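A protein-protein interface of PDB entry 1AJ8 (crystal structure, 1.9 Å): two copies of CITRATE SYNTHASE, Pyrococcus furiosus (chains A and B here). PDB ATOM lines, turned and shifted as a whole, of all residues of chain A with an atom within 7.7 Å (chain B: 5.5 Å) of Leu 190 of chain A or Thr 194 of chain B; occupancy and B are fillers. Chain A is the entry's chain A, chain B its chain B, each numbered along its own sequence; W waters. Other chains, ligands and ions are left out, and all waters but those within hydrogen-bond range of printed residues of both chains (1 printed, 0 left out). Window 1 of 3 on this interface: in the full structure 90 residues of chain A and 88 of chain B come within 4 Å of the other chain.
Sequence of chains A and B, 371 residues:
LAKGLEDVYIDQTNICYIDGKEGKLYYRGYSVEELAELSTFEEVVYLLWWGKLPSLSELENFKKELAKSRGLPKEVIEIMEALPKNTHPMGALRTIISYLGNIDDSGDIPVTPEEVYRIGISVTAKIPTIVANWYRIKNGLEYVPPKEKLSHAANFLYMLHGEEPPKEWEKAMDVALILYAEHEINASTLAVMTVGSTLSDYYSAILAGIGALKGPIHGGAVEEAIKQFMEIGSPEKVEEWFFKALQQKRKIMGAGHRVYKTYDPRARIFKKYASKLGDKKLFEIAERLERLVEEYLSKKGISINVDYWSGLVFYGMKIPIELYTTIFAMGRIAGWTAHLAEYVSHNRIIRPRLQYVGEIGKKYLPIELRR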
ATOM      1  N   GLY A   4      30.684 -26.423  26.990  1.00  0.00           N
ATOM      2  CA  GLY A   4      29.469 -26.286  27.767  1.00  0.00           C
ATOM      3  C   GLY A   4      28.535 -25.332  27.055  1.00  0.00           C
ATOM      4  O   GLY A   4      27.483 -24.975  27.579  1.00  0.00           O
ATOM      5  N   LEU A   5      28.916 -24.938  25.840  1.00  0.00           N
ATOM      6  CA  LEU A   5      28.138 -23.998  25.034  1.00  0.00           C
ATOM      7  C   LEU A   5      27.926 -22.719  25.823  1.00  0.00           C
ATOM      8  O   LEU A   5      26.951 -22.004  25.619  1.00  0.00           O
ATOM      9  CB  LEU A   5      26.782 -24.590  24.653  1.00  0.00           C
ATOM     10  CG  LEU A   5      26.729 -25.452  23.392  1.00  0.00           C
ATOM     11  CD1 LEU A   5      25.302 -25.905  23.158  1.00  0.00           C
ATOM     12  CD2 LEU A   5      27.234 -24.665  22.193  1.00  0.00           C
ATOM     13  N   ILE A  10      21.577 -19.652  21.022  1.00  0.00           N
ATOM     14  CA  ILE A  10      21.098 -20.513  19.950  1.00  0.00           C
ATOM     15  C   ILE A  10      19.830 -20.105  19.215  1.00  0.00           C
ATOM     16  O   ILE A  10      19.452 -20.736  18.228  1.00  0.00           O
ATOM     17  CB  ILE A  10      20.947 -21.973  20.472  1.00  0.00           C
ATOM     18  CG1 ILE A  10      19.588 -22.169  21.141  1.00  0.00           C
ATOM     19  CG2 ILE A  10      22.060 -22.281  21.480  1.00  0.00           C
ATOM     20  CD1 ILE A  10      19.100 -23.608  21.078  1.00  0.00           C
ATOM     21  N   GLU A 184      14.659 -20.193  30.946  1.00  0.00           N
ATOM     22  CA  GLU A 184      15.384 -20.053  29.687  1.00  0.00           C
ATOM     23  C   GLU A 184      15.925 -21.397  29.200  1.00  0.00           C
ATOM     24  O   GLU A 184      15.277 -22.428  29.384  1.00  0.00           O
ATOM     25  CB  GLU A 184      16.517 -19.034  29.865  1.00  0.00           C
ATOM     26  CG  GLU A 184      16.837 -18.193  28.632  1.00  0.00           C
ATOM     27  CD  GLU A 184      18.334 -18.044  28.437  1.00  0.00           C
ATOM     28  OE1 GLU A 184      19.044 -19.049  28.624  1.00  0.00           O
ATOM     29  OE2 GLU A 184      18.810 -16.935  28.110  1.00  0.00           O
ATOM     30  N   ILE A 185      17.117 -21.395  28.604  1.00  0.00           N
ATOM     31  CA  ILE A 185      17.680 -22.630  28.061  1.00  0.00           C
ATOM     32  C   ILE A 185      18.707 -23.374  28.924  1.00  0.00           C
ATOM     33  O   ILE A 185      19.892 -23.486  28.585  1.00  0.00           O
ATOM     34  CB  ILE A 185      18.236 -22.377  26.608  1.00  0.00           C
ATOM     35  CG1 ILE A 185      18.519 -23.707  25.907  1.00  0.00           C
ATOM     36  CG2 ILE A 185      19.468 -21.495  26.649  1.00  0.00           C
ATOM     37  CD1 ILE A 185      18.606 -23.587  24.386  1.00  0.00           C
ATOM     38  N   ASN A 186      18.227 -23.891  30.053  1.00  0.00           N
ATOM     39  CA  ASN A 186      19.050 -24.676  30.962  1.00  0.00           C
ATOM     40  C   ASN A 186      19.241 -26.007  30.230  1.00  0.00           C
ATOM     41  O   ASN A 186      18.661 -26.222  29.162  1.00  0.00           O
ATOM     42  CB  ASN A 186      18.299 -24.913  32.269  1.00  0.00           C
ATOM     43  CG  ASN A 186      16.851 -25.289  32.036  1.00  0.00           C
ATOM     44  OD1 ASN A 186      16.509 -26.467  31.955  1.00  0.00           O
ATOM     45  ND2 ASN A 186      15.993 -24.285  31.912  1.00  0.00           N
ATOM     46  N   ALA A 187      20.036 -26.902  30.808  1.00  0.00           N
ATOM     47  CA  ALA A 187      20.307 -28.197  30.186  1.00  0.00           C
ATOM     48  C   ALA A 187      19.068 -29.013  29.814  1.00  0.00           C
ATOM     49  O   ALA A 187      18.985 -29.522  28.695  1.00  0.00           O
ATOM     50  CB  ALA A 187      21.227 -29.027  31.088  1.00  0.00           C
ATOM     51  N   SER A 188      18.110 -29.148  30.734  1.00  0.00           N
ATOM     52  CA  SER A 188      16.912 -29.927  30.436  1.00  0.00           C
ATOM     53  C   SER A 188      16.092 -29.293  29.310  1.00  0.00           C
ATOM     54  O   SER A 188      15.583 -29.997  28.433  1.00  0.00           O
ATOM     55  CB  SER A 188      16.052 -30.136  31.706  1.00  0.00           C
ATOM     56  OG  SER A 188      15.488 -28.934  32.203  1.00  0.00           O
ATOM     57  N   THR A 189      15.968 -27.967  29.317  1.00  0.00           N
ATOM     58  CA  THR A 189      15.216 -27.293  28.263  1.00  0.00           C
ATOM     59  C   THR A 189      15.960 -27.425  26.923  1.00  0.00           C
ATOM     60  O   THR A 189      15.337 -27.561  25.876  1.00  0.00           O
ATOM     61  CB  THR A 189      14.975 -25.814  28.625  1.00  0.00           C
ATOM     62  OG1 THR A 189      14.069 -25.754  29.736  1.00  0.00           O
ATOM     63  CG2 THR A 189      14.374 -25.048  27.449  1.00  0.00           C
ATOM     64  N   LEU A 190      17.288 -27.401  26.951  1.00  0.00           N
ATOM     65  CA  LEU A 190      18.046 -27.561  25.707  1.00  0.00           C
ATOM     66  C   LEU A 190      17.776 -28.961  25.134  1.00  0.00           C
ATOM     67  O   LEU A 190      17.553 -29.116  23.934  1.00  0.00           O
ATOM     68  CB  LEU A 190      19.552 -27.392  25.956  1.00  0.00           C
ATOM     69  CG  LEU A 190      20.464 -27.882  24.811  1.00  0.00           C
ATOM     70  CD1 LEU A 190      20.193 -27.065  23.544  1.00  0.00           C
ATOM     71  CD2 LEU A 190      21.932 -27.773  25.219  1.00  0.00           C
ATOM     72  N   ALA A 191      17.793 -29.975  25.999  1.00  0.00           N
ATOM     73  CA  ALA A 191      17.557 -31.353  25.571  1.00  0.00           C
ATOM     74  C   ALA A 191      16.181 -31.484  24.934  1.00  0.00           C
ATOM     75  O   ALA A 191      16.017 -32.165  23.919  1.00  0.00           O
ATOM     76  CB  ALA A 191      17.688 -32.309  26.762  1.00  0.00           C
ATOM     77  N   VAL A 192      15.187 -30.835  25.532  1.00  0.00           N
ATOM     78  CA  VAL A 192      13.825 -30.861  25.008  1.00  0.00           C
ATOM     79  C   VAL A 192      13.803 -30.219  23.620  1.00  0.00           C
ATOM     80  O   VAL A 192      13.205 -30.754  22.688  1.00  0.00           O
ATOM     81  CB  VAL A 192      12.861 -30.066  25.928  1.00  0.00           C
ATOM     82  CG1 VAL A 192      11.548 -29.777  25.209  1.00  0.00           C
ATOM     83  CG2 VAL A 192      12.600 -30.857  27.195  1.00  0.00           C
ATOM     84  N   MET A 193      14.455 -29.067  23.499  1.00  0.00           N
ATOM     85  CA  MET A 193      14.505 -28.340  22.236  1.00  0.00           C
ATOM     86  C   MET A 193      15.283 -29.085  21.145  1.00  0.00           C
ATOM     87  O   MET A 193      14.909 -29.030  19.974  1.00  0.00           O
ATOM     88  CB  MET A 193      15.102 -26.947  22.462  1.00  0.00           C
ATOM     89  CG  MET A 193      14.169 -25.997  23.210  1.00  0.00           C
ATOM     90  SD  MET A 193      15.029 -24.566  23.841  1.00  0.00           S
ATOM     91  CE  MET A 193      15.223 -23.599  22.329  1.00  0.00           C
ATOM     92  N   THR A 194      16.348 -29.786  21.527  1.00  0.00           N
ATOM     93  CA  THR A 194      17.154 -30.546  20.558  1.00  0.00           C
ATOM     94  C   THR A 194      16.327 -31.667  19.936  1.00  0.00           C
ATOM     95  O   THR A 194      16.357 -31.876  18.721  1.00  0.00           O
ATOM     96  CB  THR A 194      18.421 -31.153  21.215  1.00  0.00           C
ATOM     97  OG1 THR A 194      19.210 -30.103  21.785  1.00  0.00           O
ATOM     98  CG2 THR A 194      19.274 -31.881  20.181  1.00  0.00           C
ATOM     99  N   VAL A 195      15.590 -32.390  20.772  1.00  0.00           N
ATOM    100  CA  VAL A 195      14.729 -33.468  20.300  1.00  0.00           C
ATOM    101  C   VAL A 195      13.641 -32.854  19.416  1.00  0.00           C
ATOM    102  O   VAL A 195      13.311 -33.378  18.353  1.00  0.00           O
ATOM    103  CB  VAL A 195      14.064 -34.222  21.490  1.00  0.00           C
ATOM    104  CG1 VAL A 195      13.003 -35.179  20.981  1.00  0.00           C
ATOM    105  CG2 VAL A 195      15.112 -34.997  22.264  1.00  0.00           C
ATOM    106  N   GLY A 196      13.088 -31.730  19.858  1.00  0.00           N
ATOM    107  CA  GLY A 196      12.052 -31.077  19.084  1.00  0.00           C
ATOM    108  C   GLY A 196      12.543 -30.593  17.728  1.00  0.00           C
ATOM    109  O   GLY A 196      11.774 -30.576  16.760  1.00  0.00           O
ATOM    110  N   SER A 197      13.818 -30.209  17.653  1.00  0.00           N
ATOM    111  CA  SER A 197      14.397 -29.703  16.409  1.00  0.00           C
ATOM    112  C   SER A 197      14.487 -30.743  15.283  1.00  0.00           C
ATOM    113  O   SER A 197      14.779 -30.394  14.133  1.00  0.00           O
ATOM    114  CB  SER A 197      15.776 -29.090  16.675  1.00  0.00           C
ATOM    115  OG  SER A 197      16.772 -30.085  16.801  1.00  0.00           O
ATOM    116  N   ALA A 205      10.425 -35.526  23.321  1.00  0.00           N
ATOM    117  CA  ALA A 205      11.087 -34.297  23.725  1.00  0.00           C
ATOM    118  C   ALA A 205      11.050 -34.114  25.242  1.00  0.00           C
ATOM    119  O   ALA A 205      12.085 -33.855  25.862  1.00  0.00           O
ATOM    120  CB  ALA A 205      10.445 -33.092  23.031  1.00  0.00           C
ATOM    121  N   ALA A 208      13.455 -36.260  27.238  1.00  0.00           N
ATOM    122  CA  ALA A 208      14.852 -35.823  27.258  1.00  0.00           C
ATOM    123  C   ALA A 208      15.012 -34.808  28.397  1.00  0.00           C
ATOM    124  O   ALA A 208      16.045 -34.754  29.074  1.00  0.00           O
ATOM    125  CB  ALA A 208      15.228 -35.178  25.906  1.00  0.00           C
ATOM    126  N   GLY A 209      13.981 -33.994  28.589  1.00  0.00           N
ATOM    127  CA  GLY A 209      14.009 -33.011  29.656  1.00  0.00           C
ATOM    128  C   GLY A 209      14.074 -33.730  30.994  1.00  0.00           C
ATOM    129  O   GLY A 209      14.901 -33.400  31.847  1.00  0.00           O
ATOM    130  N   GLY A 211      15.102 -36.738  31.654  1.00  0.00           N
ATOM    131  CA  GLY A 211      16.401 -37.366  31.805  1.00  0.00           C
ATOM    132  C   GLY A 211      17.474 -36.384  32.232  1.00  0.00           C
ATOM    133  O   GLY A 211      18.292 -36.686  33.102  1.00  0.00           O
ATOM    134  N   ALA A 212      17.481 -35.200  31.628  1.00  0.00           N
ATOM    135  CA  ALA A 212      18.487 -34.208  31.979  1.00  0.00           C
ATOM    136  C   ALA A 212      18.245 -33.616  33.365  1.00  0.00           C
ATOM    137  O   ALA A 212      19.182 -33.461  34.145  1.00  0.00           O
ATOM    138  CB  ALA A 212      18.522 -33.093  30.935  1.00  0.00           C
ATOM    139  N   LEU A 213      16.993 -33.281  33.663  1.00  0.00           N
ATOM    140  CA  LEU A 213      16.646 -32.692  34.955  1.00  0.00           C
ATOM    141  C   LEU A 213      17.045 -33.599  36.114  1.00  0.00           C
ATOM    142  O   LEU A 213      17.401 -33.132  37.196  1.00  0.00           O
ATOM    143  CB  LEU A 213      15.146 -32.410  35.020  1.00  0.00           C
ATOM    144  CG  LEU A 213      14.728 -31.480  36.165  1.00  0.00           C
ATOM    145  CD1 LEU A 213      15.365 -30.114  35.969  1.00  0.00           C
ATOM    146  CD2 LEU A 213      13.216 -31.364  36.209  1.00  0.00           C
ATOM    147  N   HIS A 218      22.050 -30.914  38.082  1.00  0.00           N
ATOM    148  CA  HIS A 218      20.966 -30.138  37.504  1.00  0.00           C
ATOM    149  C   HIS A 218      19.839 -30.228  38.536  1.00  0.00           C
ATOM    150  O   HIS A 218      20.091 -30.080  39.727  1.00  0.00           O
ATOM    151  CB  HIS A 218      20.488 -30.669  36.142  1.00  0.00           C
ATOM    152  CG  HIS A 218      19.623 -29.690  35.406  1.00  0.00           C
ATOM    153  ND1 HIS A 218      18.935 -30.005  34.252  1.00  0.00           N
ATOM    154  CD2 HIS A 218      19.332 -28.393  35.671  1.00  0.00           C
ATOM    155  CE1 HIS A 218      18.262 -28.944  33.839  1.00  0.00           C
ATOM    156  NE2 HIS A 218      18.486 -27.952  34.683  1.00  0.00           N
ATOM    157  N   TRP A 336       9.214 -26.254  29.626  1.00  0.00           N
ATOM    158  CA  TRP A 336       9.607 -27.168  28.555  1.00  0.00           C
ATOM    159  C   TRP A 336       8.601 -27.079  27.401  1.00  0.00           C
ATOM    160  O   TRP A 336       8.980 -27.047  26.231  1.00  0.00           O
ATOM    161  CB  TRP A 336       9.642 -28.614  29.051  1.00  0.00           C
ATOM    162  CG  TRP A 336      10.799 -28.965  29.929  1.00  0.00           C
ATOM    163  CD1 TRP A 336      11.989 -28.305  30.037  1.00  0.00           C
ATOM    164  CD2 TRP A 336      10.862 -30.061  30.846  1.00  0.00           C
ATOM    165  NE1 TRP A 336      12.789 -28.922  30.966  1.00  0.00           N
ATOM    166  CE2 TRP A 336      12.121 -30.003  31.480  1.00  0.00           C
ATOM    167  CE3 TRP A 336       9.972 -31.087  31.196  1.00  0.00           C
ATOM    168  CZ2 TRP A 336      12.517 -30.935  32.450  1.00  0.00           C
ATOM    169  CZ3 TRP A 336      10.364 -32.013  32.162  1.00  0.00           C
ATOM    170  CH2 TRP A 336      11.628 -31.929  32.777  1.00  0.00           C
ATOM    171  N   HIS A 339       8.968 -23.678  25.496  1.00  0.00           N
ATOM    172  CA  HIS A 339      10.143 -23.645  24.633  1.00  0.00           C
ATOM    173  C   HIS A 339      10.059 -24.578  23.429  1.00  0.00           C
ATOM    174  O   HIS A 339      10.528 -24.235  22.343  1.00  0.00           O
ATOM    175  CB  HIS A 339      11.405 -23.939  25.452  1.00  0.00           C
ATOM    176  CG  HIS A 339      11.977 -22.721  26.103  1.00  0.00           C
ATOM    177  ND1 HIS A 339      11.752 -22.407  27.426  1.00  0.00           N
ATOM    178  CD2 HIS A 339      12.719 -21.706  25.597  1.00  0.00           C
ATOM    179  CE1 HIS A 339      12.328 -21.251  27.706  1.00  0.00           C
ATOM    180  NE2 HIS A 339      12.922 -20.805  26.612  1.00  0.00           N
ATOM    181  N   ILE A 350      19.166 -28.656  15.481  1.00  0.00           N
ATOM    182  CA  ILE A 350      20.305 -28.232  16.281  1.00  0.00           C
ATOM    183  C   ILE A 350      21.391 -29.270  16.045  1.00  0.00           C
ATOM    184  O   ILE A 350      21.277 -30.415  16.480  1.00  0.00           O
ATOM    185  CB  ILE A 350      19.935 -28.158  17.779  1.00  0.00           C
ATOM    186  CG1 ILE A 350      18.753 -27.189  17.957  1.00  0.00           C
ATOM    187  CG2 ILE A 350      21.140 -27.707  18.591  1.00  0.00           C
ATOM    188  CD1 ILE A 350      18.252 -27.035  19.388  1.00  0.00           C
ATOM    189  N   THR B 189      23.032 -37.324  19.049  1.00  0.00           N
ATOM    190  CA  THR B 189      24.206 -37.476  19.891  1.00  0.00           C
ATOM    191  C   THR B 189      24.336 -36.265  20.820  1.00  0.00           C
ATOM    192  O   THR B 189      24.779 -36.402  21.956  1.00  0.00           O
ATOM    193  CB  THR B 189      25.481 -37.655  19.028  1.00  0.00           C
ATOM    194  OG1 THR B 189      25.454 -38.955  18.425  1.00  0.00           O
ATOM    195  CG2 THR B 189      26.739 -37.537  19.876  1.00  0.00           C
ATOM    196  N   LEU B 190      23.941 -35.085  20.345  1.00  0.00           N
ATOM    197  CA  LEU B 190      24.008 -33.887  21.180  1.00  0.00           C
ATOM    198  C   LEU B 190      23.014 -34.048  22.338  1.00  0.00           C
ATOM    199  O   LEU B 190      23.312 -33.678  23.479  1.00  0.00           O
ATOM    200  CB  LEU B 190      23.656 -32.632  20.373  1.00  0.00           C
ATOM    201  CG  LEU B 190      23.319 -31.387  21.207  1.00  0.00           C
ATOM    202  CD1 LEU B 190      24.537 -30.965  22.006  1.00  0.00           C
ATOM    203  CD2 LEU B 190      22.864 -30.256  20.303  1.00  0.00           C
ATOM    204  N   ALA B 191      21.840 -34.605  22.042  1.00  0.00           N
ATOM    205  CA  ALA B 191      20.818 -34.815  23.067  1.00  0.00           C
ATOM    206  C   ALA B 191      21.362 -35.764  24.127  1.00  0.00           C
ATOM    207  O   ALA B 191      21.213 -35.529  25.327  1.00  0.00           O
ATOM    208  CB  ALA B 191      19.543 -35.386  22.439  1.00  0.00           C
ATOM    209  N   VAL B 192      22.007 -36.833  23.678  1.00  0.00           N
ATOM    210  CA  VAL B 192      22.598 -37.817  24.578  1.00  0.00           C
ATOM    211  C   VAL B 192      23.664 -37.165  25.470  1.00  0.00           C
ATOM    212  O   VAL B 192      23.678 -37.365  26.686  1.00  0.00           O
ATOM    213  CB  VAL B 192      23.239 -38.978  23.773  1.00  0.00           C
ATOM    214  CG1 VAL B 192      24.113 -39.840  24.674  1.00  0.00           C
ATOM    215  CG2 VAL B 192      22.143 -39.826  23.130  1.00  0.00           C
ATOM    216  N   MET B 193      24.547 -36.377  24.867  1.00  0.00           N
ATOM    217  CA  MET B 193      25.608 -35.720  25.617  1.00  0.00           C
ATOM    218  C   MET B 193      25.072 -34.653  26.571  1.00  0.00           C
ATOM    219  O   MET B 193      25.644 -34.425  27.638  1.00  0.00           O
ATOM    220  CB  MET B 193      26.622 -35.103  24.651  1.00  0.00           C
ATOM    221  CG  MET B 193      27.404 -36.145  23.840  1.00  0.00           C
ATOM    222  SD  MET B 193      28.316 -35.428  22.451  1.00  0.00           S
ATOM    223  CE  MET B 193      29.460 -34.379  23.302  1.00  0.00           C
ATOM    224  N   THR B 194      23.975 -34.003  26.193  1.00  0.00           N
ATOM    225  CA  THR B 194      23.385 -32.966  27.042  1.00  0.00           C
ATOM    226  C   THR B 194      22.846 -33.594  28.329  1.00  0.00           C
ATOM    227  O   THR B 194      23.066 -33.074  29.425  1.00  0.00           O
ATOM    228  CB  THR B 194      22.263 -32.215  26.300  1.00  0.00           C
ATOM    229  OG1 THR B 194      22.823 -31.546  25.168  1.00  0.00           O
ATOM    230  CG2 THR B 194      21.618 -31.168  27.198  1.00  0.00           C
ATOM    231  N   VAL B 195      22.147 -34.713  28.202  1.00  0.00           N
ATOM    232  CA  VAL B 195      21.622 -35.391  29.378  1.00  0.00           C
ATOM    233  C   VAL B 195      22.802 -35.908  30.195  1.00  0.00           C
ATOM    234  O   VAL B 195      22.809 -35.813  31.425  1.00  0.00           O
ATOM    235  CB  VAL B 195      20.720 -36.579  28.987  1.00  0.00           C
ATOM    236  CG1 VAL B 195      20.352 -37.389  30.235  1.00  0.00           C
ATOM    237  CG2 VAL B 195      19.477 -36.068  28.286  1.00  0.00           C
ATOM    238  N   GLY B 196      23.807 -36.442  29.502  1.00  0.00           N
ATOM    239  CA  GLY B 196      24.982 -36.961  30.180  1.00  0.00           C
ATOM    240  C   GLY B 196      25.739 -35.878  30.934  1.00  0.00           C
ATOM    241  O   GLY B 196      26.340 -36.133  31.983  1.00  0.00           O
ATOM    242  N   SER B 197      25.695 -34.659  30.405  1.00  0.00           N
ATOM    243  CA  SER B 197      26.394 -33.541  31.015  1.00  0.00           C
ATOM    244  C   SER B 197      25.856 -33.113  32.387  1.00  0.00           C
ATOM    245  O   SER B 197      26.505 -32.325  33.081  1.00  0.00           O
ATOM    246  CB  SER B 197      26.423 -32.344  30.053  1.00  0.00           C
ATOM    247  OG  SER B 197      25.238 -31.575  30.116  1.00  0.00           O
ATOM    248  N   THR B 198      24.683 -33.614  32.781  1.00  0.00           N
ATOM    249  CA  THR B 198      24.134 -33.270  34.097  1.00  0.00           C
ATOM    250  C   THR B 198      24.453 -34.416  35.045  1.00  0.00           C
ATOM    251  O   THR B 198      24.052 -34.409  36.215  1.00  0.00           O
ATOM    252  CB  THR B 198      22.606 -33.063  34.077  1.00  0.00           C
ATOM    253  OG1 THR B 198      21.957 -34.307  33.798  1.00  0.00           O
ATOM    254  CG2 THR B 198      22.216 -32.039  33.028  1.00  0.00           C
ATOM    255  N   ILE B 350      26.154 -28.743  29.671  1.00  0.00           N
ATOM    256  CA  ILE B 350      25.892 -28.034  28.427  1.00  0.00           C
ATOM    257  C   ILE B 350      24.695 -27.140  28.689  1.00  0.00           C
ATOM    258  O   ILE B 350      23.572 -27.617  28.862  1.00  0.00           O
ATOM    259  CB  ILE B 350      25.602 -29.027  27.279  1.00  0.00           C
ATOM    260  CG1 ILE B 350      26.823 -29.932  27.074  1.00  0.00           C
ATOM    261  CG2 ILE B 350      25.302 -28.272  25.982  1.00  0.00           C
ATOM    262  CD1 ILE B 350      26.652 -30.983  25.978  1.00  0.00           C
ATOM    263  N   ARG B 351      24.940 -25.837  28.736  1.00  0.00           N
ATOM    264  CA  ARG B 351      23.875 -24.888  29.024  1.00  0.00           C
ATOM    265  C   ARG B 351      24.189 -23.535  28.371  1.00  0.00           C
ATOM    266  O   ARG B 351      24.985 -22.739  28.876  1.00  0.00           O
ATOM    267  CB  ARG B 351      23.687 -24.812  30.560  1.00  0.00           C
ATOM    268  CG  ARG B 351      23.605 -23.441  31.190  1.00  0.00           C
ATOM    269  CD  ARG B 351      22.220 -23.102  31.695  1.00  0.00           C
ATOM    270  NE  ARG B 351      21.673 -22.036  30.881  1.00  0.00           N
ATOM    271  CZ  ARG B 351      20.624 -21.282  31.180  1.00  0.00           C
ATOM    272  NH1 ARG B 351      19.946 -21.436  32.306  1.00  0.00           N
ATOM    273  NH2 ARG B 351      20.244 -20.368  30.309  1.00  0.00           N
ATOM    274  N   PRO B 352      23.577 -23.281  27.202  1.00  0.00           N
ATOM    275  CA  PRO B 352      23.744 -22.056  26.417  1.00  0.00           C
ATOM    276  C   PRO B 352      22.771 -20.966  26.844  1.00  0.00           C
ATOM    277  O   PRO B 352      22.267 -20.986  27.962  1.00  0.00           O
ATOM    278  CB  PRO B 352      23.477 -22.525  24.992  1.00  0.00           C
ATOM    279  CG  PRO B 352      22.443 -23.610  25.161  1.00  0.00           C
ATOM    280  CD  PRO B 352      22.654 -24.222  26.540  1.00  0.00           C
HETATM  281  O   HOH W   1      20.642 -31.416  23.586  1.00  0.00           O
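O of Gly 4 of chain A lies within hydrogen-bond range of N of Arg 351 of chain B, 2.9 Å away. The side-chain carboxylate of Glu 184 of chain A is in salt-bridge range of the guanidinium group of Arg 351 of chain B. The backbone carbonyl oxygen of Ile 185 of chain A lies within hydrogen-bond range of the guanidinium group of Arg 351 of chain B (3.2 Å). The backbone carbonyl oxygen of Ala 212 of chain A sits at hydrogen-bond distance from the side-chain hydroxyl of Thr 198 of chain B (2.9 Å).
ND2 of Asn 186 of chain A is in hydrogen-bond range of O of Glu 184 of chain A, 3.2 Å away. The side-chain amide oxygen (OD1) of Asn 186 of chain A sits at hydrogen-bond distance from the side-chain hydroxyl (OG) of Ser 188 of chain A. The side-chain amide oxygen (OD1) of Asn 186 of chain A lies within hydrogen-bond range of the backbone NH (N) of Thr 189 of chain A. The backbone carbonyl oxygen (O) of Thr 194 of chain A sits at hydrogen-bond distance from the side-chain hydroxyl (OG) of Ser 197 of chain A, at 2.7 Å. A ring nitrogen (ND1) of His 218 of chain A is in hydrogen-bond range of the backbone carbonyl oxygen (O) of Ala 212 of chain A, 3.5 Å away. O of Leu 190 of chain B sits at hydrogen-bond distance from OG1 of Thr 194 of chain B (2.8 Å).
Gly 4 of chain A touches Ile 350 of chain B. O of Arg 351 of chain B touches O of Leu 5 of chain A (3.9 Å). OE1 of Glu 184 of chain A touches O of Pro 352 of chain B, 3.8 Å away. Ile 185 of chain A touches Pro 352 of chain B (CG2 to O, 3.1 Å). Asn 186 of chain A touches Arg 351 of chain B (CA to CD, 3.6 Å). Thr 194 of chain B touches Ala 187 of chain A (CG2 to O, 3.4 Å). CB of Ala 187 of chain A touches CG2 of Thr 198 of chain B, at 3.7 Å. Ile 350 of chain B touches Ala 187 of chain A (O to CB, 3.5 Å). CD2 of Leu 190 of chain B touches CG2 of Thr 194 of chain A, 3.9 Å away. Ile 350 of chain A touches Leu 190 of chain B (CG2 to CD2, 3.5 Å).
Of chain B, only Thr 194, Ile 350 and Pro 352 come within 4 Å of Leu 190 of chain A. Thr 194 of chain B touches just these residues of chain A: Ala 187 and Leu 190. Printed residues of chain B within 4 Å of Asn 186 of chain A: Arg 351 (3.6 Å). Of the printed residues of chain B, Ile 350 of chain A touches Leu 190. Printed residues of chain B within 4 Å of Ala 208 of chain A: Val 195 (3.8 Å). Printed residues of chain B within 4 Å of Gly 211 of chain A: Val 195. Printed residues of chain B within 4 Å of Leu 5 of chain A: Ile 350 (3.7 Å), Arg 351 (3.9 Å) and Pro 352 (3.3 Å). Ser 197 of chain A touches none of the printed residues of chain B. The nearest residue of chain B that does not touch Leu 190 of chain A is Arg 351 of chain B (5.0 Å). The nearest printed residue of chain A that does not touch Pro 352 of chain B is Gly 4 of chain A (4.3 Å).
Hydrophobic or aromatic side chains of chain A that line the printed part of chain B: Leu 5, Ile 10, Ile 185, Ala 187, Leu 190, His 218 and Ile 350. Along chain A the printed residues that touch a printed residue of chain B span positions 4 to 350. Hydrophobic or aromatic side chains of chain B within 4 Å of the printed part of chain A: Leu 190, Val 195, Ile 350 and Pro 352.
Leu 190 of chain A touches Thr 194 of chain B, and with the chains exchanged Thr 194 of chain A touches Leu 190 of chain B. Leu 190 of chain A touches Ile 350 of chain B, and with the chains exchanged Ile 350 of chain A touches Leu 190 of chain B. Of the 24 pairs that touch across the chains among the printed residues, 4 have their exchanged pair printed and touching as well.
Water W1 lies within hydrogen-bond range of the side-chain hydroxyl (OG1) of Thr 194 of chain A (2.6 Å) and the side-chain hydroxyl (OG1) of Thr 194 of chain B (2.7 Å).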
